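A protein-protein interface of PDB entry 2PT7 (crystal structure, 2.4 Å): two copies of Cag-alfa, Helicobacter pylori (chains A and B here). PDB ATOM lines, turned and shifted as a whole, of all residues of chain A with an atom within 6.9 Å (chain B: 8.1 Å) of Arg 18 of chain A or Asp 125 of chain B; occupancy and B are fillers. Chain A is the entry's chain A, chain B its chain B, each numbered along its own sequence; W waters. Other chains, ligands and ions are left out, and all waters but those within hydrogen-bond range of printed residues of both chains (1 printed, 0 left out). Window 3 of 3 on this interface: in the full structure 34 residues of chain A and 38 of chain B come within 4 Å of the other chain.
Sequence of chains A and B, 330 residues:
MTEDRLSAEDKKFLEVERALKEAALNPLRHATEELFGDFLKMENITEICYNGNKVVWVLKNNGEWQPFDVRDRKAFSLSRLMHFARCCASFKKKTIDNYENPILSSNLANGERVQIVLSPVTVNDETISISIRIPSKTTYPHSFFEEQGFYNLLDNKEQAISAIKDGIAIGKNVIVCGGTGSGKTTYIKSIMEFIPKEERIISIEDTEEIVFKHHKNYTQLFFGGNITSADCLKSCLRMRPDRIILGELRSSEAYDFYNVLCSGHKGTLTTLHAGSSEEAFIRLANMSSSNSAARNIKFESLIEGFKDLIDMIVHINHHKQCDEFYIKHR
OD2 of Asp 125 of chain B lies within salt-bridge range of NZ of Lys 21 of chain A.
NE of Arg 18 of chain A lies within salt-bridge range of OD1 of Asp 125 of chain B, at 3.0 Å.
The side-chain carboxylate (OE2) of Glu 17 of chain A lies within hydrogen-bond range of the side-chain hydroxyl (OH) of Tyr 99 of chain B (3.2 Å).
The guanidinium group (NH2) of Arg 18 of chain A lies within salt-bridge range of the side-chain carboxylate (OE2) of Glu 126 of chain B, at 2.6 Å.
No position is printed for both chains.
Of the 13 printed residues of chain A, 4 touch a printed residue of chain B.
Along chain A the printed residues that touch a printed residue of chain B span positions 14 to 21.
Of the 14 printed residues of chain B, 4 touch a printed residue of chain A.
Hydrophobic or aromatic side chains of chain B within 4 Å of the printed part of chain A: Leu 78 and Tyr 99.
Among the printed residues, Asp or Glu carboxylates within 4 Å of a Lys or Arg side-chain nitrogen of the other chain: Arg 18 of chain A with Asp 125 of chain B (3.0 Å), Arg 18 of chain A with Glu 126 of chain B (2.6 Å) and Lys 21 of chain A with Asp 125 of chain B (2.5 Å).
NH1 of Arg 18 of chain A is in salt-bridge range of OE1 of Glu 15 of chain A, at 2.8 Å.
The side-chain amide oxygen (OD1) of Asn 124 of chain B lies within hydrogen-bond range of the backbone NH (N) of Glu 126 of chain B (3.0 Å).
Water W1 bridges OE2 of Glu 17 of chain A (2.4 Å) and OD1 of Asn 98 of chain B (2.7 Å).
CD2 of Leu 14 of chain A touches CD1 of Leu 78 of chain B, 3.7 Å away.
CD1 of Leu 14 of chain A touches OD2 of Asp 125 of chain B, at 3.9 Å.
Arg 18 of chain A touches just these residues of chain B: Asp 125 (3.0 Å) and Glu 126 (2.6 Å).
Asp 125 of chain B touches just these residues of chain A: Leu 14, Arg 18 and Lys 21.
No residue of chain B comes within 4 Å of Ala 19 of chain A.
Printed residues of chain A within 4 Å of Leu 78 of chain B: Leu 14.
Of the printed residues of chain A, Tyr 99 of chain B touches Glu 17 (3.2 Å).
Of the printed residues of chain B, Lys 21 of chain A touches Asp 125 (2.5 Å).
Of the printed residues of chain B, Leu 14 of chain A touches Leu 78 and Asp 125.
Of the printed residues of chain A, Glu 126 of chain B touches Arg 18 (2.6 Å).
The nearest residue of chain A that does not touch Asp 125 of chain B is Glu 17 of chain A (5.4 Å).
The nearest printed residue of chain A that does not touch Leu 78 of chain B is Arg 18 of chain A (5.9 Å).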
ATOM      1  N   LYS A  11      25.615 -19.845  -4.028  1.00  0.00           N
ATOM      2  CA  LYS A  11      26.669 -20.129  -3.054  1.00  0.00           C
ATOM      3  C   LYS A  11      26.285 -19.551  -1.695  1.00  0.00           C
ATOM      4  O   LYS A  11      26.579 -20.135  -0.651  1.00  0.00           O
ATOM      5  CB  LYS A  11      27.987 -19.510  -3.530  1.00  0.00           C
ATOM      6  CG  LYS A  11      29.224 -20.366  -3.333  1.00  0.00           C
ATOM      7  CD  LYS A  11      30.405 -19.750  -4.080  1.00  0.00           C
ATOM      8  CE  LYS A  11      31.615 -20.675  -4.098  1.00  0.00           C
ATOM      9  NZ  LYS A  11      32.265 -20.795  -2.760  1.00  0.00           N
ATOM     10  N   PHE A  13      23.014 -18.912  -0.734  1.00  0.00           N
ATOM     11  CA  PHE A  13      21.835 -19.634  -0.256  1.00  0.00           C
ATOM     12  C   PHE A  13      22.172 -21.005   0.347  1.00  0.00           C
ATOM     13  O   PHE A  13      21.454 -21.493   1.219  1.00  0.00           O
ATOM     14  CB  PHE A  13      20.773 -19.769  -1.360  1.00  0.00           C
ATOM     15  CG  PHE A  13      19.484 -20.384  -0.884  1.00  0.00           C
ATOM     16  CD1 PHE A  13      19.192 -21.719  -1.153  1.00  0.00           C
ATOM     17  CD2 PHE A  13      18.574 -19.636  -0.142  1.00  0.00           C
ATOM     18  CE1 PHE A  13      18.006 -22.298  -0.698  1.00  0.00           C
ATOM     19  CE2 PHE A  13      17.385 -20.207   0.320  1.00  0.00           C
ATOM     20  CZ  PHE A  13      17.102 -21.540   0.043  1.00  0.00           C
ATOM     21  N   LEU A  14      23.260 -21.613  -0.120  1.00  0.00           N
ATOM     22  CA  LEU A  14      23.752 -22.862   0.453  1.00  0.00           C
ATOM     23  C   LEU A  14      24.122 -22.689   1.935  1.00  0.00           C
ATOM     24  O   LEU A  14      23.877 -23.579   2.753  1.00  0.00           O
ATOM     25  CB  LEU A  14      24.926 -23.404  -0.374  1.00  0.00           C
ATOM     26  CG  LEU A  14      25.599 -24.696   0.115  1.00  0.00           C
ATOM     27  CD1 LEU A  14      24.818 -25.815   0.080  1.00  0.00           C
ATOM     28  CD2 LEU A  14      26.531 -25.173  -0.723  1.00  0.00           C
ATOM     29  N   GLU A  15      24.680 -21.528   2.270  1.00  0.00           N
ATOM     30  CA  GLU A  15      25.007 -21.173   3.654  1.00  0.00           C
ATOM     31  C   GLU A  15      23.772 -20.939   4.528  1.00  0.00           C
ATOM     32  O   GLU A  15      23.821 -21.155   5.737  1.00  0.00           O
ATOM     33  CB  GLU A  15      25.936 -19.954   3.694  1.00  0.00           C
ATOM     34  CG  GLU A  15      27.367 -20.244   3.211  1.00  0.00           C
ATOM     35  CD  GLU A  15      27.973 -21.501   3.834  1.00  0.00           C
ATOM     36  OE1 GLU A  15      28.299 -22.442   3.077  1.00  0.00           O
ATOM     37  OE2 GLU A  15      28.115 -21.557   5.074  1.00  0.00           O
ATOM     38  N   VAL A  16      22.676 -20.498   3.908  1.00  0.00           N
ATOM     39  CA  VAL A  16      21.374 -20.395   4.576  1.00  0.00           C
ATOM     40  C   VAL A  16      20.825 -21.789   4.904  1.00  0.00           C
ATOM     41  O   VAL A  16      20.294 -22.010   5.994  1.00  0.00           O
ATOM     42  CB  VAL A  16      20.342 -19.587   3.728  1.00  0.00           C
ATOM     43  CG1 VAL A  16      18.975 -19.508   4.426  1.00  0.00           C
ATOM     44  CG2 VAL A  16      20.862 -18.193   3.443  1.00  0.00           C
ATOM     45  N   GLU A  17      20.977 -22.716   3.957  1.00  0.00           N
ATOM     46  CA  GLU A  17      20.548 -24.110   4.119  1.00  0.00           C
ATOM     47  C   GLU A  17      21.314 -24.837   5.221  1.00  0.00           C
ATOM     48  O   GLU A  17      20.714 -25.527   6.048  1.00  0.00           O
ATOM     49  CB  GLU A  17      20.682 -24.873   2.800  1.00  0.00           C
ATOM     50  CG  GLU A  17      19.755 -24.379   1.707  1.00  0.00           C
ATOM     51  CD  GLU A  17      20.000 -25.055   0.371  1.00  0.00           C
ATOM     52  OE1 GLU A  17      21.176 -25.204  -0.026  1.00  0.00           O
ATOM     53  OE2 GLU A  17      19.009 -25.431  -0.287  1.00  0.00           O
ATOM     54  N   ARG A  18      22.635 -24.661   5.223  1.00  0.00           N
ATOM     55  CA  ARG A  18      23.528 -25.231   6.240  1.00  0.00           C
ATOM     56  C   ARG A  18      23.236 -24.714   7.651  1.00  0.00           C
ATOM     57  O   ARG A  18      23.282 -25.474   8.618  1.00  0.00           O
ATOM     58  CB  ARG A  18      24.990 -24.966   5.874  1.00  0.00           C
ATOM     59  CG  ARG A  18      25.509 -25.863   4.770  1.00  0.00           C
ATOM     60  CD  ARG A  18      26.831 -25.387   4.218  1.00  0.00           C
ATOM     61  NE  ARG A  18      27.369 -26.361   3.275  1.00  0.00           N
ATOM     62  CZ  ARG A  18      28.444 -26.177   2.514  1.00  0.00           C
ATOM     63  NH1 ARG A  18      29.125 -25.037   2.559  1.00  0.00           N
ATOM     64  NH2 ARG A  18      28.835 -27.144   1.697  1.00  0.00           N
ATOM     65  N   ALA A  19      22.927 -23.424   7.756  1.00  0.00           N
ATOM     66  CA  ALA A  19      22.572 -22.812   9.034  1.00  0.00           C
ATOM     67  C   ALA A  19      21.238 -23.336   9.574  1.00  0.00           C
ATOM     68  O   ALA A  19      21.097 -23.554  10.772  1.00  0.00           O
ATOM     69  CB  ALA A  19      22.552 -21.286   8.917  1.00  0.00           C
ATOM     70  N   LEU A  20      20.271 -23.544   8.683  1.00  0.00           N
ATOM     71  CA  LEU A  20      18.978 -24.104   9.073  1.00  0.00           C
ATOM     72  C   LEU A  20      19.026 -25.605   9.380  1.00  0.00           C
ATOM     73  O   LEU A  20      18.283 -26.072  10.243  1.00  0.00           O
ATOM     74  CB  LEU A  20      17.886 -23.781   8.043  1.00  0.00           C
ATOM     75  CG  LEU A  20      17.442 -22.308   7.960  1.00  0.00           C
ATOM     76  CD1 LEU A  20      16.389 -22.076   7.160  1.00  0.00           C
ATOM     77  CD2 LEU A  20      16.818 -21.837   9.087  1.00  0.00           C
ATOM     78  N   LYS A  21      19.893 -26.347   8.683  1.00  0.00           N
ATOM     79  CA  LYS A  21      20.142 -27.765   9.002  1.00  0.00           C
ATOM     80  C   LYS A  21      20.761 -27.906  10.382  1.00  0.00           C
ATOM     81  O   LYS A  21      20.353 -28.763  11.164  1.00  0.00           O
ATOM     82  CB  LYS A  21      21.073 -28.428   7.987  1.00  0.00           C
ATOM     83  CG  LYS A  21      20.461 -28.749   6.642  1.00  0.00           C
ATOM     84  CD  LYS A  21      21.522 -29.344   5.725  1.00  0.00           C
ATOM     85  CE  LYS A  21      21.323 -28.909   4.289  1.00  0.00           C
ATOM     86  NZ  LYS A  21      22.612 -28.937   3.539  1.00  0.00           N
ATOM     87  N   GLU A  22      21.750 -27.054  10.660  1.00  0.00           N
ATOM     88  CA  GLU A  22      22.454 -27.037  11.933  1.00  0.00           C
ATOM     89  C   GLU A  22      21.520 -26.666  13.088  1.00  0.00           C
ATOM     90  O   GLU A  22      21.589 -27.259  14.166  1.00  0.00           O
ATOM     91  CB  GLU A  22      23.664 -26.094  11.864  1.00  0.00           C
ATOM     92  CG  GLU A  22      24.501 -26.056  13.136  1.00  0.00           C
ATOM     93  CD  GLU A  22      25.914 -25.547  12.904  1.00  0.00           C
ATOM     94  OE1 GLU A  22      26.719 -26.298  12.300  1.00  0.00           O
ATOM     95  OE2 GLU A  22      26.221 -24.411  13.343  1.00  0.00           O
ATOM     96  N   ALA A  23      20.641 -25.697  12.849  1.00  0.00           N
ATOM     97  CA  ALA A  23      19.616 -25.303  13.819  1.00  0.00           C
ATOM     98  C   ALA A  23      18.694 -26.463  14.207  1.00  0.00           C
ATOM     99  O   ALA A  23      18.333 -26.606  15.369  1.00  0.00           O
ATOM    100  CB  ALA A  23      18.805 -24.127  13.284  1.00  0.00           C
ATOM    101  N   ARG A  29      22.138 -32.760  19.065  1.00  0.00           N
ATOM    102  CA  ARG A  29      23.590 -32.732  19.246  1.00  0.00           C
ATOM    103  C   ARG A  29      23.982 -32.314  20.662  1.00  0.00           C
ATOM    104  O   ARG A  29      24.961 -32.813  21.208  1.00  0.00           O
ATOM    105  CB  ARG A  29      24.264 -31.825  18.209  1.00  0.00           C
ATOM    106  CG  ARG A  29      24.232 -32.370  16.787  1.00  0.00           C
ATOM    107  CD  ARG A  29      25.497 -31.994  16.010  1.00  0.00           C
ATOM    108  NE  ARG A  29      25.306 -30.858  15.112  1.00  0.00           N
ATOM    109  CZ  ARG A  29      25.408 -30.920  13.787  1.00  0.00           C
ATOM    110  NH1 ARG A  29      25.711 -32.071  13.188  1.00  0.00           N
ATOM    111  NH2 ARG A  29      25.206 -29.828  13.055  1.00  0.00           N
ATOM    112  N   LEU B  78      28.871 -26.069  -8.440  1.00  0.00           N
ATOM    113  CA  LEU B  78      27.702 -26.630  -7.784  1.00  0.00           C
ATOM    114  C   LEU B  78      26.417 -26.008  -8.327  1.00  0.00           C
ATOM    115  O   LEU B  78      25.428 -26.701  -8.512  1.00  0.00           O
ATOM    116  CB  LEU B  78      27.786 -26.410  -6.268  1.00  0.00           C
ATOM    117  CG  LEU B  78      27.442 -27.570  -5.319  1.00  0.00           C
ATOM    118  CD1 LEU B  78      27.144 -27.019  -3.927  1.00  0.00           C
ATOM    119  CD2 LEU B  78      26.281 -28.438  -5.790  1.00  0.00           C
ATOM    120  N   MET B  82      23.550 -27.750 -10.639  1.00  0.00           N
ATOM    121  CA  MET B  82      22.206 -27.681 -10.079  1.00  0.00           C
ATOM    122  C   MET B  82      21.194 -27.004 -11.010  1.00  0.00           C
ATOM    123  O   MET B  82      20.023 -27.386 -11.045  1.00  0.00           O
ATOM    124  CB  MET B  82      22.243 -26.980  -8.725  1.00  0.00           C
ATOM    125  CG  MET B  82      21.104 -27.384  -7.818  1.00  0.00           C
ATOM    126  SD  MET B  82      21.063 -29.138  -7.413  1.00  0.00           S
ATOM    127  CE  MET B  82      22.443 -29.189  -6.279  1.00  0.00           C
ATOM    128  N   ASN B  98      16.628 -31.136  -2.977  1.00  0.00           N
ATOM    129  CA  ASN B  98      17.296 -31.821  -1.872  1.00  0.00           C
ATOM    130  C   ASN B  98      16.327 -32.263  -0.780  1.00  0.00           C
ATOM    131  O   ASN B  98      16.736 -32.500   0.360  1.00  0.00           O
ATOM    132  CB  ASN B  98      18.400 -30.938  -1.280  1.00  0.00           C
ATOM    133  CG  ASN B  98      19.392 -30.469  -2.328  1.00  0.00           C
ATOM    134  OD1 ASN B  98      19.355 -29.316  -2.748  1.00  0.00           O
ATOM    135  ND2 ASN B  98      20.272 -31.357  -2.762  1.00  0.00           N
ATOM    136  N   TYR B  99      15.046 -32.389  -1.129  1.00  0.00           N
ATOM    137  CA  TYR B  99      14.007 -32.627  -0.116  1.00  0.00           C
ATOM    138  C   TYR B  99      13.158 -33.866  -0.393  1.00  0.00           C
ATOM    139  O   TYR B  99      13.557 -34.972  -0.021  1.00  0.00           O
ATOM    140  CB  TYR B  99      13.212 -31.329   0.166  1.00  0.00           C
ATOM    141  CG  TYR B  99      14.182 -30.202   0.483  1.00  0.00           C
ATOM    142  CD1 TYR B  99      14.595 -29.305  -0.509  1.00  0.00           C
ATOM    143  CD2 TYR B  99      14.768 -30.101   1.750  1.00  0.00           C
ATOM    144  CE1 TYR B  99      15.534 -28.316  -0.235  1.00  0.00           C
ATOM    145  CE2 TYR B  99      15.697 -29.120   2.035  1.00  0.00           C
ATOM    146  CZ  TYR B  99      16.078 -28.226   1.042  1.00  0.00           C
ATOM    147  OH  TYR B  99      17.004 -27.246   1.338  1.00  0.00           O
ATOM    148  N   LEU B 118      20.829 -36.273  -5.923  1.00  0.00           N
ATOM    149  CA  LEU B 118      21.296 -35.184  -5.077  1.00  0.00           C
ATOM    150  C   LEU B 118      21.362 -35.618  -3.618  1.00  0.00           C
ATOM    151  O   LEU B 118      20.867 -36.690  -3.258  1.00  0.00           O
ATOM    152  CB  LEU B 118      20.355 -33.980  -5.187  1.00  0.00           C
ATOM    153  CG  LEU B 118      19.948 -33.436  -6.559  1.00  0.00           C
ATOM    154  CD1 LEU B 118      18.986 -32.284  -6.375  1.00  0.00           C
ATOM    155  CD2 LEU B 118      21.161 -33.017  -7.407  1.00  0.00           C
ATOM    156  N   SER B 119      21.985 -34.777  -2.794  1.00  0.00           N
ATOM    157  CA  SER B 119      21.931 -34.882  -1.343  1.00  0.00           C
ATOM    158  C   SER B 119      20.451 -34.776  -0.907  1.00  0.00           C
ATOM    159  O   SER B 119      19.709 -33.984  -1.485  1.00  0.00           O
ATOM    160  CB  SER B 119      22.765 -33.740  -0.741  1.00  0.00           C
ATOM    161  OG  SER B 119      22.847 -33.816   0.674  1.00  0.00           O
ATOM    162  N   PRO B 120      20.020 -35.532   0.129  1.00  0.00           N
ATOM    163  CA  PRO B 120      20.774 -36.370   1.060  1.00  0.00           C
ATOM    164  C   PRO B 120      20.968 -37.828   0.632  1.00  0.00           C
ATOM    165  O   PRO B 120      21.396 -38.644   1.444  1.00  0.00           O
ATOM    166  CB  PRO B 120      19.930 -36.289   2.354  1.00  0.00           C
ATOM    167  CG  PRO B 120      18.516 -36.055   1.880  1.00  0.00           C
ATOM    168  CD  PRO B 120      18.576 -35.564   0.440  1.00  0.00           C
ATOM    169  N   THR B 122      23.081 -38.609  -1.982  1.00  0.00           N
ATOM    170  CA  THR B 122      24.532 -38.630  -2.177  1.00  0.00           C
ATOM    171  C   THR B 122      25.216 -38.321  -0.836  1.00  0.00           C
ATOM    172  O   THR B 122      24.546 -37.974   0.148  1.00  0.00           O
ATOM    173  CB  THR B 122      25.001 -37.631  -3.264  1.00  0.00           C
ATOM    174  OG1 THR B 122      24.606 -36.306  -2.908  1.00  0.00           O
ATOM    175  CG2 THR B 122      24.433 -37.992  -4.635  1.00  0.00           C
ATOM    176  N   VAL B 123      26.542 -38.437  -0.809  1.00  0.00           N
ATOM    177  CA  VAL B 123      27.308 -38.406   0.447  1.00  0.00           C
ATOM    178  C   VAL B 123      27.316 -37.053   1.193  1.00  0.00           C
ATOM    179  O   VAL B 123      27.396 -37.025   2.426  1.00  0.00           O
ATOM    180  CB  VAL B 123      28.741 -38.984   0.245  1.00  0.00           C
ATOM    181  CG1 VAL B 123      29.616 -38.047  -0.612  1.00  0.00           C
ATOM    182  CG2 VAL B 123      29.391 -39.325   1.590  1.00  0.00           C
ATOM    183  N   ASN B 124      27.216 -35.944   0.462  1.00  0.00           N
ATOM    184  CA  ASN B 124      27.149 -34.625   1.091  1.00  0.00           C
ATOM    185  C   ASN B 124      26.489 -33.521   0.253  1.00  0.00           C
ATOM    186  O   ASN B 124      26.139 -33.720  -0.913  1.00  0.00           O
ATOM    187  CB  ASN B 124      28.541 -34.171   1.593  1.00  0.00           C
ATOM    188  CG  ASN B 124      29.578 -34.054   0.476  1.00  0.00           C
ATOM    189  OD1 ASN B 124      29.339 -33.438  -0.557  1.00  0.00           O
ATOM    190  ND2 ASN B 124      30.742 -34.634   0.698  1.00  0.00           N
ATOM    191  N   ASP B 125      26.318 -32.376   0.911  1.00  0.00           N
ATOM    192  CA  ASP B 125      25.911 -31.071   0.355  1.00  0.00           C
ATOM    193  C   ASP B 125      26.368 -30.697  -1.050  1.00  0.00           C
ATOM    194  O   ASP B 125      25.661 -29.983  -1.772  1.00  0.00           O
ATOM    195  CB  ASP B 125      26.464 -29.966   1.280  1.00  0.00           C
ATOM    196  CG  ASP B 125      25.405 -29.314   2.085  1.00  0.00           C
ATOM    197  OD1 ASP B 125      25.705 -28.806   3.176  1.00  0.00           O
ATOM    198  OD2 ASP B 125      24.249 -29.307   1.626  1.00  0.00           O
ATOM    199  N   GLU B 126      27.578 -31.115  -1.399  1.00  0.00           N
ATOM    200  CA  GLU B 126      28.248 -30.614  -2.598  1.00  0.00           C
ATOM    201  C   GLU B 126      28.441 -31.703  -3.657  1.00  0.00           C
ATOM    202  O   GLU B 126      29.187 -31.505  -4.631  1.00  0.00           O
ATOM    203  CB  GLU B 126      29.590 -29.982  -2.211  1.00  0.00           C
ATOM    204  CG  GLU B 126      29.470 -28.798  -1.262  1.00  0.00           C
ATOM    205  CD  GLU B 126      30.813 -28.329  -0.686  1.00  0.00           C
ATOM    206  OE1 GLU B 126      31.849 -29.004  -0.911  1.00  0.00           O
ATOM    207  OE2 GLU B 126      30.829 -27.279   0.006  1.00  0.00           O
ATOM    208  N   THR B 127      27.763 -32.838  -3.467  1.00  0.00           N
ATOM    209  CA  THR B 127      27.887 -33.987  -4.371  1.00  0.00           C
ATOM    210  C   THR B 127      26.631 -34.193  -5.225  1.00  0.00           C
ATOM    211  O   THR B 127      25.533 -34.416  -4.706  1.00  0.00           O
ATOM    212  CB  THR B 127      28.205 -35.283  -3.596  1.00  0.00           C
ATOM    213  OG1 THR B 127      29.305 -35.054  -2.713  1.00  0.00           O
ATOM    214  CG2 THR B 127      28.543 -36.436  -4.544  1.00  0.00           C
ATOM    215  N   ILE B 128      26.809 -34.102  -6.536  1.00  0.00           N
ATOM    216  CA  ILE B 128      25.747 -34.364  -7.498  1.00  0.00           C
ATOM    217  C   ILE B 128      26.212 -35.493  -8.400  1.00  0.00           C
ATOM    218  O   ILE B 128      27.287 -35.408  -8.998  1.00  0.00           O
ATOM    219  CB  ILE B 128      25.406 -33.106  -8.357  1.00  0.00           C
ATOM    220  CG1 ILE B 128      24.962 -31.940  -7.466  1.00  0.00           C
ATOM    221  CG2 ILE B 128      24.333 -33.427  -9.416  1.00  0.00           C
ATOM    222  CD1 ILE B 128      24.880 -30.612  -8.195  1.00  0.00           C
HETATM  223  O   HOH W   1      18.567 -26.836  -2.202  1.00  0.00           O
